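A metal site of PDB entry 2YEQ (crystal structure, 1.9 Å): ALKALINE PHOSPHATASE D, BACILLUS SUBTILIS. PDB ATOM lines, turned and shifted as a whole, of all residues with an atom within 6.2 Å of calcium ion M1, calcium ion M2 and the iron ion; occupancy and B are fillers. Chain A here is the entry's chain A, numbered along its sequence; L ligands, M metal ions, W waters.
Within 4 Å of calcium ion M2: Asp 151, Asp 209, Asp 210 and Asp 380.
The nearest printed residue that does not touch calcium ion M2 is His 211 (4.2 Å).
The side-chain hydroxyl (OH) of Tyr 154 sits close to the side-chain hydroxyl (OG) of Ser 412, at 2.6 Å.
The side-chain carboxylate of Asp 151 sits at hydrogen-bond distance from the backbone NH of His 211, at 3.1 Å.
O of Asp 151 sits at hydrogen-bond distance from N of Gln 125.
NE of Arg 279 is in salt-bridge range of OD1 of Asp 209, at 2.8 Å.
OD1 of Asn 215 lies close to NE2 of His 211, 3.0 Å away.
The backbone NH (N) of Cys 124 sits at hydrogen-bond distance from the backbone carbonyl oxygen (O) of Gly 150, 2.9 Å away.
The side-chain sulfur (SG) of Cys 124 lies close to the side-chain hydroxyl (OG) of Ser 123, 3.8 Å away.
A ring nitrogen (NE2) of His 510 lies within hydrogen-bond range of a ring nitrogen (NE2) of His 211.
NE2 of His 211 touches calcium ion M1, 3.7 Å away.
The iron ion is bound by the side-chain hydroxyl (OH) of Tyr 154 (2.0 Å), the side-chain carboxylate (OD2) of Asp 151 (2.2 Å), a ring nitrogen (NE2) of His 382 (2.2 Å), an oxygen (O3) of the ligand (2.3 Å), an oxygen (O4) of the ligand (2.3 Å) and the side-chain sulfur (SG) of Cys 124 (2.5 Å).
Calcium ion M1 is bound by water W1, the side-chain carboxylate of Asp 210, the side-chain amide oxygen of Asn 215, the side-chain amide oxygen of Asn 216, water W2 and an oxygen (O2) of the ligand.
Calcium ion M1 has six donor atoms within binding distance.
Water W2 lies within hydrogen-bond range of the side-chain carboxylate (OD2) of Asp 350 (2.8 Å) and the guanidinium group (NH2) of Arg 279 (3.5 Å).
Of the 23 residues printed, 4 come within 4 Å of the iron ion.
Calcium ion M2 is bound by OD2 of Asp 209 (2.3 Å), O2 of the ligand (2.3 Å), OD1 of Asp 380 (2.4 Å), OD1 of Asp 210 (2.4 Å), OD2 of Asp 151 (2.5 Å), water W3 (2.6 Å) and O4 of the ligand (2.6 Å).
Slightly farther from calcium ion M2 lies the side-chain carboxylate (OD1) of Asp 151 (2.9 Å).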
ATOM      1  N   SER A 123     -15.405  20.055  -3.773  1.00  0.00           N
ATOM      2  CA  SER A 123     -14.897  18.783  -4.315  1.00  0.00           C
ATOM      3  C   SER A 123     -14.642  17.841  -3.173  1.00  0.00           C
ATOM      4  O   SER A 123     -14.594  18.252  -2.014  1.00  0.00           O
ATOM      5  CB  SER A 123     -13.597  19.048  -5.080  1.00  0.00           C
ATOM      6  OG  SER A 123     -12.580  19.446  -4.192  1.00  0.00           O
ATOM      7  N   CYS A 124     -14.438  16.556  -3.503  1.00  0.00           N
ATOM      8  CA  CYS A 124     -13.769  15.612  -2.600  1.00  0.00           C
ATOM      9  C   CYS A 124     -14.504  15.336  -1.272  1.00  0.00           C
ATOM     10  O   CYS A 124     -14.141  15.809  -0.171  1.00  0.00           O
ATOM     11  CB  CYS A 124     -12.291  15.987  -2.389  1.00  0.00           C
ATOM     12  SG  CYS A 124     -11.260  15.916  -3.938  1.00  0.00           S
ATOM     13  N   GLN A 125     -15.510  14.479  -1.389  1.00  0.00           N
ATOM     14  CA  GLN A 125     -16.408  14.202  -0.276  1.00  0.00           C
ATOM     15  C   GLN A 125     -16.428  12.730   0.152  1.00  0.00           C
ATOM     16  O   GLN A 125     -17.501  12.149   0.299  1.00  0.00           O
ATOM     17  CB  GLN A 125     -17.816  14.701  -0.617  1.00  0.00           C
ATOM     18  CG  GLN A 125     -18.428  14.167  -1.894  1.00  0.00           C
ATOM     19  CD  GLN A 125     -19.489  15.054  -2.429  1.00  0.00           C
ATOM     20  OE1 GLN A 125     -19.392  16.294  -2.327  1.00  0.00           O
ATOM     21  NE2 GLN A 125     -20.511  14.464  -3.053  1.00  0.00           N
ATOM     22  N   GLY A 150     -15.256  17.577  -8.652  1.00  0.00           N
ATOM     23  CA  GLY A 150     -14.899  16.128  -8.755  1.00  0.00           C
ATOM     24  C   GLY A 150     -14.793  15.399  -7.431  1.00  0.00           C
ATOM     25  O   GLY A 150     -14.850  16.003  -6.364  1.00  0.00           O
ATOM     26  N   ASP A 151     -14.585  14.076  -7.542  1.00  0.00           N
ATOM     27  CA  ASP A 151     -14.592  13.165  -6.435  1.00  0.00           C
ATOM     28  C   ASP A 151     -15.892  13.352  -5.654  1.00  0.00           C
ATOM     29  O   ASP A 151     -15.887  13.416  -4.429  1.00  0.00           O
ATOM     30  CB  ASP A 151     -13.358  13.304  -5.559  1.00  0.00           C
ATOM     31  CG  ASP A 151     -12.058  12.900  -6.262  1.00  0.00           C
ATOM     32  OD1 ASP A 151     -12.086  12.557  -7.455  1.00  0.00           O
ATOM     33  OD2 ASP A 151     -10.989  12.982  -5.588  1.00  0.00           O
ATOM     34  N   TYR A 154     -16.400   8.192  -4.146  1.00  0.00           N
ATOM     35  CA  TYR A 154     -15.166   7.423  -4.181  1.00  0.00           C
ATOM     36  C   TYR A 154     -15.582   5.955  -4.401  1.00  0.00           C
ATOM     37  O   TYR A 154     -16.704   5.564  -4.043  1.00  0.00           O
ATOM     38  CB  TYR A 154     -14.325   7.567  -2.897  1.00  0.00           C
ATOM     39  CG  TYR A 154     -13.649   8.921  -2.778  1.00  0.00           C
ATOM     40  CD1 TYR A 154     -14.398  10.090  -2.574  1.00  0.00           C
ATOM     41  CD2 TYR A 154     -12.276   9.049  -2.916  1.00  0.00           C
ATOM     42  CE1 TYR A 154     -13.798  11.338  -2.498  1.00  0.00           C
ATOM     43  CE2 TYR A 154     -11.641  10.302  -2.836  1.00  0.00           C
ATOM     44  CZ  TYR A 154     -12.413  11.438  -2.639  1.00  0.00           C
ATOM     45  OH  TYR A 154     -11.822  12.666  -2.537  1.00  0.00           O
ATOM     46  N   TYR A 161      -9.262   3.117   1.853  1.00  0.00           N
ATOM     47  CA  TYR A 161      -8.721   4.471   1.835  1.00  0.00           C
ATOM     48  C   TYR A 161      -9.067   5.121   3.167  1.00  0.00           C
ATOM     49  O   TYR A 161     -10.168   5.643   3.347  1.00  0.00           O
ATOM     50  CB  TYR A 161      -9.320   5.242   0.677  1.00  0.00           C
ATOM     51  CG  TYR A 161      -8.899   6.702   0.597  1.00  0.00           C
ATOM     52  CD1 TYR A 161      -7.679   7.152   1.098  1.00  0.00           C
ATOM     53  CD2 TYR A 161      -9.746   7.628   0.019  1.00  0.00           C
ATOM     54  CE1 TYR A 161      -7.324   8.472   1.022  1.00  0.00           C
ATOM     55  CE2 TYR A 161      -9.387   8.955  -0.077  1.00  0.00           C
ATOM     56  CZ  TYR A 161      -8.182   9.370   0.423  1.00  0.00           C
ATOM     57  OH  TYR A 161      -7.858  10.703   0.356  1.00  0.00           O
ATOM     58  N   ASP A 209     -13.875  14.268 -11.461  1.00  0.00           N
ATOM     59  CA  ASP A 209     -12.441  14.025 -11.503  1.00  0.00           C
ATOM     60  C   ASP A 209     -12.246  12.494 -11.570  1.00  0.00           C
ATOM     61  O   ASP A 209     -12.997  11.837 -12.305  1.00  0.00           O
ATOM     62  CB  ASP A 209     -11.685  14.666 -10.319  1.00  0.00           C
ATOM     63  CG  ASP A 209     -10.162  14.663 -10.533  1.00  0.00           C
ATOM     64  OD1 ASP A 209      -9.698  14.842 -11.701  1.00  0.00           O
ATOM     65  OD2 ASP A 209      -9.412  14.420  -9.515  1.00  0.00           O
ATOM     66  N   ASP A 210     -11.311  11.932 -10.822  1.00  0.00           N
ATOM     67  CA  ASP A 210     -10.966  10.502 -11.023  1.00  0.00           C
ATOM     68  C   ASP A 210     -11.862   9.535 -10.279  1.00  0.00           C
ATOM     69  O   ASP A 210     -12.217   8.492 -10.829  1.00  0.00           O
ATOM     70  CB  ASP A 210      -9.492  10.170 -10.702  1.00  0.00           C
ATOM     71  CG  ASP A 210      -9.014  10.708  -9.381  1.00  0.00           C
ATOM     72  OD1 ASP A 210      -9.607  11.705  -8.857  1.00  0.00           O
ATOM     73  OD2 ASP A 210      -8.016  10.173  -8.844  1.00  0.00           O
ATOM     74  N   HIS A 211     -12.236   9.882  -9.042  1.00  0.00           N
ATOM     75  CA  HIS A 211     -12.908   8.935  -8.176  1.00  0.00           C
ATOM     76  C   HIS A 211     -14.353   8.630  -8.520  1.00  0.00           C
ATOM     77  O   HIS A 211     -14.905   7.663  -7.991  1.00  0.00           O
ATOM     78  CB  HIS A 211     -12.735   9.316  -6.725  1.00  0.00           C
ATOM     79  CG  HIS A 211     -11.367   9.032  -6.181  1.00  0.00           C
ATOM     80  ND1 HIS A 211     -10.912   7.748  -5.951  1.00  0.00           N
ATOM     81  CD2 HIS A 211     -10.394   9.866  -5.745  1.00  0.00           C
ATOM     82  CE1 HIS A 211      -9.706   7.815  -5.391  1.00  0.00           C
ATOM     83  NE2 HIS A 211      -9.361   9.082  -5.279  1.00  0.00           N
ATOM     84  N   ASN A 215      -9.443   5.791  -8.914  1.00  0.00           N
ATOM     85  CA  ASN A 215      -8.266   6.623  -8.628  1.00  0.00           C
ATOM     86  C   ASN A 215      -7.254   6.743  -9.789  1.00  0.00           C
ATOM     87  O   ASN A 215      -6.764   5.719 -10.314  1.00  0.00           O
ATOM     88  CB  ASN A 215      -7.500   6.095  -7.414  1.00  0.00           C
ATOM     89  CG  ASN A 215      -6.445   7.084  -6.922  1.00  0.00           C
ATOM     90  OD1 ASN A 215      -6.761   8.259  -6.638  1.00  0.00           O
ATOM     91  ND2 ASN A 215      -5.199   6.616  -6.795  1.00  0.00           N
ATOM     92  N   ASN A 216      -6.937   7.994 -10.133  1.00  0.00           N
ATOM     93  CA  ASN A 216      -5.875   8.359 -11.072  1.00  0.00           C
ATOM     94  C   ASN A 216      -5.960   7.720 -12.434  1.00  0.00           C
ATOM     95  O   ASN A 216      -4.922   7.491 -13.092  1.00  0.00           O
ATOM     96  CB  ASN A 216      -4.493   8.109 -10.460  1.00  0.00           C
ATOM     97  CG  ASN A 216      -4.085   9.200  -9.435  1.00  0.00           C
ATOM     98  OD1 ASN A 216      -4.914   9.666  -8.677  1.00  0.00           O
ATOM     99  ND2 ASN A 216      -2.805   9.580  -9.410  1.00  0.00           N
ATOM    100  N   ARG A 279      -9.927  14.472 -17.245  1.00  0.00           N
ATOM    101  CA  ARG A 279      -9.766  13.026 -17.096  1.00  0.00           C
ATOM    102  C   ARG A 279     -10.044  12.235 -18.357  1.00  0.00           C
ATOM    103  O   ARG A 279      -9.298  11.296 -18.648  1.00  0.00           O
ATOM    104  CB  ARG A 279     -10.711  12.454 -16.020  1.00  0.00           C
ATOM    105  CG  ARG A 279     -10.267  12.712 -14.637  1.00  0.00           C
ATOM    106  CD  ARG A 279      -9.030  12.013 -14.227  1.00  0.00           C
ATOM    107  NE  ARG A 279      -8.525  12.593 -12.988  1.00  0.00           N
ATOM    108  CZ  ARG A 279      -7.317  12.418 -12.470  1.00  0.00           C
ATOM    109  NH1 ARG A 279      -6.402  11.599 -13.047  1.00  0.00           N
ATOM    110  NH2 ARG A 279      -6.995  13.063 -11.363  1.00  0.00           N
ATOM    111  N   GLN A 331     -10.327  20.535 -12.425  1.00  0.00           N
ATOM    112  CA  GLN A 331     -10.132  19.522 -11.392  1.00  0.00           C
ATOM    113  C   GLN A 331      -8.896  19.632 -10.555  1.00  0.00           C
ATOM    114  O   GLN A 331      -8.930  19.343  -9.347  1.00  0.00           O
ATOM    115  CB  GLN A 331     -10.110  18.132 -12.055  1.00  0.00           C
ATOM    116  CG  GLN A 331     -11.415  17.690 -12.690  1.00  0.00           C
ATOM    117  CD  GLN A 331     -11.782  18.403 -13.974  1.00  0.00           C
ATOM    118  OE1 GLN A 331     -10.929  18.924 -14.710  1.00  0.00           O
ATOM    119  NE2 GLN A 331     -13.090  18.408 -14.282  1.00  0.00           N
ATOM    120  N   ILE A 332      -7.771  19.957 -11.202  1.00  0.00           N
ATOM    121  CA  ILE A 332      -6.473  19.675 -10.632  1.00  0.00           C
ATOM    122  C   ILE A 332      -5.548  20.923 -10.551  1.00  0.00           C
ATOM    123  O   ILE A 332      -5.746  21.925 -11.222  1.00  0.00           O
ATOM    124  CB  ILE A 332      -5.756  18.547 -11.444  1.00  0.00           C
ATOM    125  CG1 ILE A 332      -5.845  18.821 -12.936  1.00  0.00           C
ATOM    126  CG2 ILE A 332      -6.365  17.130 -11.100  1.00  0.00           C
ATOM    127  CD1 ILE A 332      -4.829  18.033 -13.787  1.00  0.00           C
ATOM    128  N   ASP A 350       0.156  13.948 -11.629  1.00  0.00           N
ATOM    129  CA  ASP A 350      -1.296  13.922 -11.918  1.00  0.00           C
ATOM    130  C   ASP A 350      -1.936  15.307 -12.061  1.00  0.00           C
ATOM    131  O   ASP A 350      -3.078  15.437 -12.505  1.00  0.00           O
ATOM    132  CB  ASP A 350      -1.999  13.128 -10.816  1.00  0.00           C
ATOM    133  CG  ASP A 350      -3.439  12.795 -11.169  1.00  0.00           C
ATOM    134  OD1 ASP A 350      -3.708  12.191 -12.241  1.00  0.00           O
ATOM    135  OD2 ASP A 350      -4.318  13.141 -10.328  1.00  0.00           O
ATOM    136  N   ASP A 380      -9.281  18.465  -5.849  1.00  0.00           N
ATOM    137  CA  ASP A 380      -8.348  17.303  -5.913  1.00  0.00           C
ATOM    138  C   ASP A 380      -7.371  17.142  -4.768  1.00  0.00           C
ATOM    139  O   ASP A 380      -7.153  16.017  -4.301  1.00  0.00           O
ATOM    140  CB  ASP A 380      -7.630  17.214  -7.272  1.00  0.00           C
ATOM    141  CG  ASP A 380      -6.772  15.931  -7.398  1.00  0.00           C
ATOM    142  OD1 ASP A 380      -7.344  14.802  -7.466  1.00  0.00           O
ATOM    143  OD2 ASP A 380      -5.520  16.084  -7.378  1.00  0.00           O
ATOM    144  N   VAL A 381      -6.825  18.248  -4.280  1.00  0.00           N
ATOM    145  CA  VAL A 381      -5.677  18.174  -3.381  1.00  0.00           C
ATOM    146  C   VAL A 381      -6.008  18.186  -1.907  1.00  0.00           C
ATOM    147  O   VAL A 381      -5.131  18.065  -1.071  1.00  0.00           O
ATOM    148  CB  VAL A 381      -4.577  19.263  -3.737  1.00  0.00           C
ATOM    149  CG1 VAL A 381      -4.225  19.171  -5.245  1.00  0.00           C
ATOM    150  CG2 VAL A 381      -5.016  20.682  -3.318  1.00  0.00           C
ATOM    151  N   HIS A 382      -7.296  18.256  -1.580  1.00  0.00           N
ATOM    152  CA  HIS A 382      -7.775  18.059  -0.199  1.00  0.00           C
ATOM    153  C   HIS A 382      -7.210  19.105   0.783  1.00  0.00           C
ATOM    154  O   HIS A 382      -6.977  18.834   1.943  1.00  0.00           O
ATOM    155  CB  HIS A 382      -7.472  16.637   0.310  1.00  0.00           C
ATOM    156  CG  HIS A 382      -8.071  15.531  -0.536  1.00  0.00           C
ATOM    157  ND1 HIS A 382      -7.767  14.207  -0.297  1.00  0.00           N
ATOM    158  CD2 HIS A 382      -8.922  15.542  -1.579  1.00  0.00           C
ATOM    159  CE1 HIS A 382      -8.407  13.443  -1.169  1.00  0.00           C
ATOM    160  NE2 HIS A 382      -9.121  14.218  -1.967  1.00  0.00           N
ATOM    161  N   SER A 409     -11.193  19.963   0.513  1.00  0.00           N
ATOM    162  CA  SER A 409     -12.193  18.918   0.354  1.00  0.00           C
ATOM    163  C   SER A 409     -13.353  19.110   1.361  1.00  0.00           C
ATOM    164  O   SER A 409     -13.150  19.656   2.448  1.00  0.00           O
ATOM    165  CB  SER A 409     -11.520  17.604   0.625  1.00  0.00           C
ATOM    166  OG  SER A 409     -10.754  17.648   1.816  1.00  0.00           O
ATOM    167  N   SER A 412     -12.637  14.631   2.426  1.00  0.00           N
ATOM    168  CA  SER A 412     -11.513  13.701   2.173  1.00  0.00           C
ATOM    169  C   SER A 412     -10.304  14.145   2.950  1.00  0.00           C
ATOM    170  O   SER A 412      -9.932  15.325   2.919  1.00  0.00           O
ATOM    171  CB  SER A 412     -11.172  13.633   0.681  1.00  0.00           C
ATOM    172  OG  SER A 412     -12.318  13.327  -0.064  1.00  0.00           O
ATOM    173  N   ARG A 506      -1.147  11.895   0.887  1.00  0.00           N
ATOM    174  CA  ARG A 506      -2.297  11.633   0.037  1.00  0.00           C
ATOM    175  C   ARG A 506      -1.999  10.487  -0.973  1.00  0.00           C
ATOM    176  O   ARG A 506      -2.779   9.553  -1.094  1.00  0.00           O
ATOM    177  CB  ARG A 506      -2.756  12.919  -0.661  1.00  0.00           C
ATOM    178  CG  ARG A 506      -4.038  12.793  -1.474  1.00  0.00           C
ATOM    179  CD  ARG A 506      -4.584  14.138  -1.873  1.00  0.00           C
ATOM    180  NE  ARG A 506      -3.603  14.922  -2.631  1.00  0.00           N
ATOM    181  CZ  ARG A 506      -3.563  15.058  -3.959  1.00  0.00           C
ATOM    182  NH1 ARG A 506      -4.468  14.494  -4.763  1.00  0.00           N
ATOM    183  NH2 ARG A 506      -2.593  15.811  -4.494  1.00  0.00           N
ATOM    184  N   HIS A 510      -3.636   6.610  -0.737  1.00  0.00           N
ATOM    185  CA  HIS A 510      -4.270   5.956  -1.882  1.00  0.00           C
ATOM    186  C   HIS A 510      -3.548   4.647  -2.295  1.00  0.00           C
ATOM    187  O   HIS A 510      -4.202   3.722  -2.773  1.00  0.00           O
ATOM    188  CB  HIS A 510      -4.312   6.897  -3.071  1.00  0.00           C
ATOM    189  CG  HIS A 510      -5.346   7.965  -2.968  1.00  0.00           C
ATOM    190  ND1 HIS A 510      -5.158   9.125  -2.240  1.00  0.00           N
ATOM    191  CD2 HIS A 510      -6.578   8.069  -3.511  1.00  0.00           C
ATOM    192  CE1 HIS A 510      -6.217   9.895  -2.349  1.00  0.00           C
ATOM    193  NE2 HIS A 510      -7.096   9.284  -3.126  1.00  0.00           N
HETATM  194  P1  LIG L   1      -7.919  12.506  -4.707  1.00  0.00           P
HETATM  195  O1  LIG L   1      -6.531  12.614  -4.213  1.00  0.00           O
HETATM  196  O2  LIG L   1      -8.102  12.047  -6.121  1.00  0.00           O
HETATM  197  O3  LIG L   1      -8.839  11.861  -3.686  1.00  0.00           O
HETATM  198  O4  LIG L   1      -8.495  13.942  -4.911  1.00  0.00           O
HETATM  199 CA    CA M   1      -6.506  10.540  -7.173  1.00  0.00          CA
HETATM  200 CA    CA M   2      -9.330  13.536  -7.391  1.00  0.00          CA
HETATM  201 FE    FE M   3     -10.401  13.580  -3.603  1.00  0.00          FE
HETATM  202  O   HOH W   1      -5.070  10.781  -5.484  1.00  0.00           O
HETATM  203  O   HOH W   2      -5.882  12.611  -8.121  1.00  0.00           O
HETATM  204  O   HOH W   3     -10.888  15.562  -7.069  1.00  0.00           O
